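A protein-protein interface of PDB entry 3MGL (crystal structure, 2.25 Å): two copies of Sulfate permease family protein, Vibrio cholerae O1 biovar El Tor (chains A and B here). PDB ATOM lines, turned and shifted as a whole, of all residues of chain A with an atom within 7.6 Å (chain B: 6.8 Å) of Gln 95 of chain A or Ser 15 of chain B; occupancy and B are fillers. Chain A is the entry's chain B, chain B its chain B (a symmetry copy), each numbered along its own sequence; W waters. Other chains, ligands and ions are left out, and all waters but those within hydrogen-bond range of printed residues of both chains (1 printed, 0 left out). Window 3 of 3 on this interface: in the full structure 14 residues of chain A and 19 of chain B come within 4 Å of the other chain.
CD of Arg 92 of chain A touches O of Ser 15 of chain B (3.4 Å).
CG2 of Thr 16 of chain B touches O of Arg 92 of chain A, 3.4 Å away.
CB of Gln 95 of chain A touches CG2 of Thr 16 of chain B, 3.9 Å away.
Lys 96 of chain A touches Thr 16 of chain B.
Gln 95 of chain A touches just these residues of chain B: Ser 15 (3.3 Å) and Thr 16 (3.9 Å).
Of chain A, only Arg 92 (3.4 Å) and Gln 95 (3.3 Å) come within 4 Å of Ser 15 of chain B.
Printed residues of chain B within 4 Å of Lys 99 of chain A: Thr 16 (3.3 Å) and Leu 17 (3.3 Å).
Of the printed residues of chain B, Lys 96 of chain A touches Thr 16 and Leu 17.
Of the printed residues of chain A, Leu 17 of chain B touches Lys 96 (2.7 Å) and Lys 99 (3.3 Å).
Printed residues of chain B within 4 Å of Arg 92 of chain A: Ser 15 (3.4 Å) and Thr 16 (3.4 Å).
Met 5 of chain B touches none of the printed residues of chain A.
Ala 100 of chain A touches none of the printed residues of chain B.
The nearest printed residue of chain B that does not touch Arg 92 of chain A is Ser 6 of chain B (4.2 Å).
The side-chain amide oxygen (OD1) of Asn 90 of chain A is in hydrogen-bond range of the backbone NH (N) of Arg 92 of chain A (2.9 Å).
No position is printed for both chains.
The side-chain hydroxyl of Ser 15 of chain B lies within hydrogen-bond range of the side-chain amide oxygen of Gln 95 of chain A, at 3.3 Å.
The side-chain amino group of Lys 96 of chain A is in hydrogen-bond range of the backbone carbonyl oxygen of Leu 17 of chain B (2.7 Å).
The backbone carbonyl oxygen of Leu 17 of chain B lies within hydrogen-bond range of the side-chain amino group of Lys 99 of chain A, 3.3 Å away.
The side-chain amino group of Lys 99 of chain A sits at hydrogen-bond distance from the side-chain hydroxyl of Thr 16 of chain B, at 3.3 Å.
Hydrophobic or aromatic side chains of chain B that line the printed part of chain A: Leu 17.
Among the printed residues, 8 pairs touch across the chains.
Among the printed residues, no Asp or Glu carboxylate lies within 4 Å of a Lys or Arg side-chain nitrogen of the other chain.
Water W1 lies within hydrogen-bond range of NZ of Lys 96 of chain A (2.8 Å) and O of Leu 17 of chain B (3.3 Å).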
ATOM      1  N   ALA A  89     -13.008  28.558  19.447  1.00  0.00           N
ATOM      2  CA  ALA A  89     -13.848  27.975  18.395  1.00  0.00           C
ATOM      3  C   ALA A  89     -14.837  27.010  19.040  1.00  0.00           C
ATOM      4  O   ALA A  89     -14.438  26.206  19.868  1.00  0.00           O
ATOM      5  CB  ALA A  89     -12.987  27.252  17.387  1.00  0.00           C
ATOM      6  N   ASN A  90     -16.126  27.100  18.716  1.00  0.00           N
ATOM      7  CA  ASN A  90     -17.066  26.094  19.225  1.00  0.00           C
ATOM      8  C   ASN A  90     -16.740  24.714  18.647  1.00  0.00           C
ATOM      9  O   ASN A  90     -15.772  24.563  17.895  1.00  0.00           O
ATOM     10  CB  ASN A  90     -18.549  26.498  19.068  1.00  0.00           C
ATOM     11  CG  ASN A  90     -19.007  26.560  17.622  1.00  0.00           C
ATOM     12  OD1 ASN A  90     -18.629  25.726  16.791  1.00  0.00           O
ATOM     13  ND2 ASN A  90     -19.854  27.541  17.321  1.00  0.00           N
ATOM     14  N   SER A  91     -17.509  23.699  18.995  1.00  0.00           N
ATOM     15  CA  SER A  91     -17.119  22.358  18.583  1.00  0.00           C
ATOM     16  C   SER A  91     -17.304  22.110  17.063  1.00  0.00           C
ATOM     17  O   SER A  91     -16.628  21.268  16.486  1.00  0.00           O
ATOM     18  CB  SER A  91     -17.836  21.302  19.419  1.00  0.00           C
ATOM     19  OG  SER A  91     -19.086  21.009  18.841  1.00  0.00           O
ATOM     20  N   ARG A  92     -18.210  22.851  16.437  1.00  0.00           N
ATOM     21  CA  ARG A  92     -18.450  22.748  15.002  1.00  0.00           C
ATOM     22  C   ARG A  92     -17.380  23.535  14.217  1.00  0.00           C
ATOM     23  O   ARG A  92     -16.743  22.999  13.303  1.00  0.00           O
ATOM     24  CB  ARG A  92     -19.882  23.212  14.688  1.00  0.00           C
ATOM     25  CG  ARG A  92     -20.117  23.795  13.305  1.00  0.00           C
ATOM     26  CD  ARG A  92     -21.631  24.069  13.038  1.00  0.00           C
ATOM     27  NE  ARG A  92     -22.102  25.294  13.695  1.00  0.00           N
ATOM     28  CZ  ARG A  92     -23.132  25.353  14.546  1.00  0.00           C
ATOM     29  NH1 ARG A  92     -23.837  24.262  14.840  1.00  0.00           N
ATOM     30  NH2 ARG A  92     -23.478  26.516  15.100  1.00  0.00           N
ATOM     31  N   VAL A  93     -17.155  24.788  14.605  1.00  0.00           N
ATOM     32  CA  VAL A  93     -16.108  25.581  13.984  1.00  0.00           C
ATOM     33  C   VAL A  93     -14.728  24.910  14.174  1.00  0.00           C
ATOM     34  O   VAL A  93     -13.942  24.877  13.233  1.00  0.00           O
ATOM     35  CB  VAL A  93     -16.116  27.052  14.453  1.00  0.00           C
ATOM     36  CG1 VAL A  93     -14.944  27.831  13.817  1.00  0.00           C
ATOM     37  CG2 VAL A  93     -17.452  27.708  14.122  1.00  0.00           C
ATOM     38  N   SER A  94     -14.473  24.339  15.357  1.00  0.00           N
ATOM     39  CA  SER A  94     -13.230  23.568  15.606  1.00  0.00           C
ATOM     40  C   SER A  94     -13.014  22.492  14.550  1.00  0.00           C
ATOM     41  O   SER A  94     -11.916  22.353  14.028  1.00  0.00           O
ATOM     42  CB  SER A  94     -13.223  22.909  16.982  1.00  0.00           C
ATOM     43  OG  SER A  94     -13.249  23.895  18.002  1.00  0.00           O
ATOM     44  N   GLN A  95     -14.074  21.746  14.243  1.00  0.00           N
ATOM     45  CA  GLN A  95     -14.010  20.725  13.214  1.00  0.00           C
ATOM     46  C   GLN A  95     -13.715  21.345  11.834  1.00  0.00           C
ATOM     47  O   GLN A  95     -12.827  20.877  11.121  1.00  0.00           O
ATOM     48  CB  GLN A  95     -15.286  19.876  13.208  1.00  0.00           C
ATOM     49  CG  GLN A  95     -15.196  18.651  12.319  1.00  0.00           C
ATOM     50  CD  GLN A  95     -16.165  17.529  12.704  1.00  0.00           C
ATOM     51  OE1 GLN A  95     -16.945  17.637  13.658  1.00  0.00           O
ATOM     52  NE2 GLN A  95     -16.104  16.436  11.960  1.00  0.00           N
ATOM     53  N   LYS A  96     -14.433  22.415  11.491  1.00  0.00           N
ATOM     54  CA  LYS A  96     -14.245  23.117  10.215  1.00  0.00           C
ATOM     55  C   LYS A  96     -12.803  23.630  10.022  1.00  0.00           C
ATOM     56  O   LYS A  96     -12.251  23.531   8.940  1.00  0.00           O
ATOM     57  CB  LYS A  96     -15.227  24.295  10.111  1.00  0.00           C
ATOM     58  CG  LYS A  96     -15.602  24.673   8.691  1.00  0.00           C
ATOM     59  CD  LYS A  96     -16.308  23.520   8.015  1.00  0.00           C
ATOM     60  CE  LYS A  96     -17.018  23.959   6.791  1.00  0.00           C
ATOM     61  NZ  LYS A  96     -18.311  24.552   7.185  1.00  0.00           N
ATOM     62  N   LEU A  97     -12.198  24.150  11.086  1.00  0.00           N
ATOM     63  CA  LEU A  97     -10.827  24.652  11.025  1.00  0.00           C
ATOM     64  C   LEU A  97      -9.798  23.563  10.713  1.00  0.00           C
ATOM     65  O   LEU A  97      -8.805  23.845  10.040  1.00  0.00           O
ATOM     66  CB  LEU A  97     -10.439  25.350  12.330  1.00  0.00           C
ATOM     67  CG  LEU A  97     -11.184  26.625  12.743  1.00  0.00           C
ATOM     68  CD1 LEU A  97     -10.696  27.071  14.102  1.00  0.00           C
ATOM     69  CD2 LEU A  97     -10.955  27.695  11.722  1.00  0.00           C
ATOM     70  N   VAL A  98     -10.027  22.347  11.230  1.00  0.00           N
ATOM     71  CA  VAL A  98      -9.176  21.196  10.921  1.00  0.00           C
ATOM     72  C   VAL A  98      -9.390  20.822   9.461  1.00  0.00           C
ATOM     73  O   VAL A  98      -8.435  20.665   8.691  1.00  0.00           O
ATOM     74  CB  VAL A  98      -9.506  19.948  11.810  1.00  0.00           C
ATOM     75  CG1 VAL A  98      -8.759  18.700  11.300  1.00  0.00           C
ATOM     76  CG2 VAL A  98      -9.200  20.209  13.296  1.00  0.00           C
ATOM     77  N   LYS A  99     -10.667  20.670   9.117  1.00  0.00           N
ATOM     78  CA  LYS A  99     -11.125  20.282   7.791  1.00  0.00           C
ATOM     79  C   LYS A  99     -10.518  21.211   6.718  1.00  0.00           C
ATOM     80  O   LYS A  99     -10.022  20.735   5.694  1.00  0.00           O
ATOM     81  CB  LYS A  99     -12.668  20.301   7.799  1.00  0.00           C
ATOM     82  CG  LYS A  99     -13.409  20.035   6.494  1.00  0.00           C
ATOM     83  CD  LYS A  99     -14.920  20.224   6.734  1.00  0.00           C
ATOM     84  CE  LYS A  99     -15.739  20.070   5.456  1.00  0.00           C
ATOM     85  NZ  LYS A  99     -17.202  20.378   5.682  1.00  0.00           N
ATOM     86  N   ALA A 100     -10.509  22.516   6.999  1.00  0.00           N
ATOM     87  CA  ALA A 100     -10.030  23.533   6.049  1.00  0.00           C
ATOM     88  C   ALA A 100      -8.504  23.677   5.966  1.00  0.00           C
ATOM     89  O   ALA A 100      -7.984  24.369   5.082  1.00  0.00           O
ATOM     90  CB  ALA A 100     -10.658  24.882   6.372  1.00  0.00           C
ATOM     91  N   GLY A 101      -7.789  23.038   6.884  1.00  0.00           N
ATOM     92  CA  GLY A 101      -6.331  23.196   6.927  1.00  0.00           C
ATOM     93  C   GLY A 101      -5.863  24.418   7.706  1.00  0.00           C
ATOM     94  O   GLY A 101      -4.681  24.729   7.699  1.00  0.00           O
ATOM     95  N   VAL A 103      -5.870  24.722  11.064  1.00  0.00           N
ATOM     96  CA  VAL A 103      -5.144  24.268  12.244  1.00  0.00           C
ATOM     97  C   VAL A 103      -3.712  23.917  11.845  1.00  0.00           C
ATOM     98  O   VAL A 103      -2.748  24.303  12.532  1.00  0.00           O
ATOM     99  CB  VAL A 103      -5.855  23.069  12.930  1.00  0.00           C
ATOM    100  CG1 VAL A 103      -4.987  22.470  14.035  1.00  0.00           C
ATOM    101  CG2 VAL A 103      -7.232  23.500  13.491  1.00  0.00           C
ATOM    102  N   MET B   5     -29.496  25.362  12.347  1.00  0.00           N
ATOM    103  CA  MET B   5     -28.520  24.724  11.510  1.00  0.00           C
ATOM    104  C   MET B   5     -28.139  23.374  12.114  1.00  0.00           C
ATOM    105  O   MET B   5     -27.999  22.399  11.382  1.00  0.00           O
ATOM    106  CB  MET B   5     -27.316  25.649  11.395  1.00  0.00           C
ATOM    107  CG  MET B   5     -26.367  25.347  10.288  1.00  0.00           C
ATOM    108  SD  MET B   5     -25.064  26.779  10.270  1.00  0.00           S
ATOM    109  CE  MET B   5     -26.246  28.212   9.666  1.00  0.00           C
ATOM    110  N   SER B   6     -28.005  23.313  13.445  1.00  0.00           N
ATOM    111  CA  SER B   6     -27.600  22.079  14.141  1.00  0.00           C
ATOM    112  C   SER B   6     -28.536  20.913  13.819  1.00  0.00           C
ATOM    113  O   SER B   6     -28.087  19.833  13.406  1.00  0.00           O
ATOM    114  CB  SER B   6     -27.494  22.303  15.678  1.00  0.00           C
ATOM    115  N   LEU B   9     -28.450  19.889  10.003  1.00  0.00           N
ATOM    116  CA  LEU B   9     -27.214  19.238   9.674  1.00  0.00           C
ATOM    117  C   LEU B   9     -27.238  17.780  10.164  1.00  0.00           C
ATOM    118  O   LEU B   9     -26.852  16.876   9.435  1.00  0.00           O
ATOM    119  CB  LEU B   9     -26.005  20.012  10.226  1.00  0.00           C
ATOM    120  CG  LEU B   9     -25.705  21.371   9.576  1.00  0.00           C
ATOM    121  CD1 LEU B   9     -24.591  22.139  10.324  1.00  0.00           C
ATOM    122  CD2 LEU B   9     -25.367  21.244   8.100  1.00  0.00           C
ATOM    123  N   ALA B  10     -27.721  17.577  11.387  1.00  0.00           N
ATOM    124  CA  ALA B  10     -27.752  16.253  12.006  1.00  0.00           C
ATOM    125  C   ALA B  10     -28.726  15.303  11.314  1.00  0.00           C
ATOM    126  O   ALA B  10     -28.449  14.111  11.224  1.00  0.00           O
ATOM    127  CB  ALA B  10     -28.043  16.354  13.496  1.00  0.00           C
ATOM    128  N   GLY B  13     -26.860  13.792   8.718  1.00  0.00           N
ATOM    129  CA  GLY B  13     -25.674  13.030   9.153  1.00  0.00           C
ATOM    130  C   GLY B  13     -24.410  13.885   9.228  1.00  0.00           C
ATOM    131  O   GLY B  13     -23.289  13.367   9.176  1.00  0.00           O
ATOM    132  N   ARG B  14     -24.600  15.195   9.385  1.00  0.00           N
ATOM    133  CA  ARG B  14     -23.507  16.175   9.339  1.00  0.00           C
ATOM    134  C   ARG B  14     -23.359  16.955  10.643  1.00  0.00           C
ATOM    135  O   ARG B  14     -24.329  17.148  11.368  1.00  0.00           O
ATOM    136  CB  ARG B  14     -23.757  17.180   8.208  1.00  0.00           C
ATOM    137  CG  ARG B  14     -23.477  16.638   6.835  1.00  0.00           C
ATOM    138  CD  ARG B  14     -23.611  17.713   5.781  1.00  0.00           C
ATOM    139  NE  ARG B  14     -23.649  17.103   4.450  1.00  0.00           N
ATOM    140  CZ  ARG B  14     -22.574  16.795   3.734  1.00  0.00           C
ATOM    141  NH1 ARG B  14     -22.725  16.241   2.535  1.00  0.00           N
ATOM    142  NH2 ARG B  14     -21.351  17.055   4.212  1.00  0.00           N
ATOM    143  N   SER B  15     -22.145  17.417  10.911  1.00  0.00           N
ATOM    144  CA  SER B  15     -21.874  18.330  12.034  1.00  0.00           C
ATOM    145  C   SER B  15     -21.508  19.746  11.566  1.00  0.00           C
ATOM    146  O   SER B  15     -21.750  20.716  12.270  1.00  0.00           O
ATOM    147  CB  SER B  15     -20.784  17.767  12.949  1.00  0.00           C
ATOM    148  OG  SER B  15     -19.836  16.992  12.213  1.00  0.00           O
ATOM    149  N   THR B  16     -20.946  19.862  10.367  1.00  0.00           N
ATOM    150  CA  THR B  16     -20.554  21.161   9.839  1.00  0.00           C
ATOM    151  C   THR B  16     -21.242  21.448   8.514  1.00  0.00           C
ATOM    152  O   THR B  16     -21.709  20.540   7.839  1.00  0.00           O
ATOM    153  CB  THR B  16     -19.030  21.248   9.630  1.00  0.00           C
ATOM    154  OG1 THR B  16     -18.629  20.263   8.674  1.00  0.00           O
ATOM    155  CG2 THR B  16     -18.286  21.039  10.951  1.00  0.00           C
ATOM    156  N   LEU B  17     -21.294  22.723   8.144  1.00  0.00           N
ATOM    157  CA  LEU B  17     -21.785  23.099   6.827  1.00  0.00           C
ATOM    158  C   LEU B  17     -20.891  22.498   5.759  1.00  0.00           C
ATOM    159  O   LEU B  17     -19.678  22.599   5.859  1.00  0.00           O
ATOM    160  CB  LEU B  17     -21.814  24.615   6.662  1.00  0.00           C
ATOM    161  CG  LEU B  17     -22.981  25.373   7.267  1.00  0.00           C
ATOM    162  CD1 LEU B  17     -22.661  26.818   7.201  1.00  0.00           C
ATOM    163  CD2 LEU B  17     -24.289  25.071   6.528  1.00  0.00           C
HETATM  164  O   HOH W   1     -18.445  25.291   4.468  1.00  0.00           O
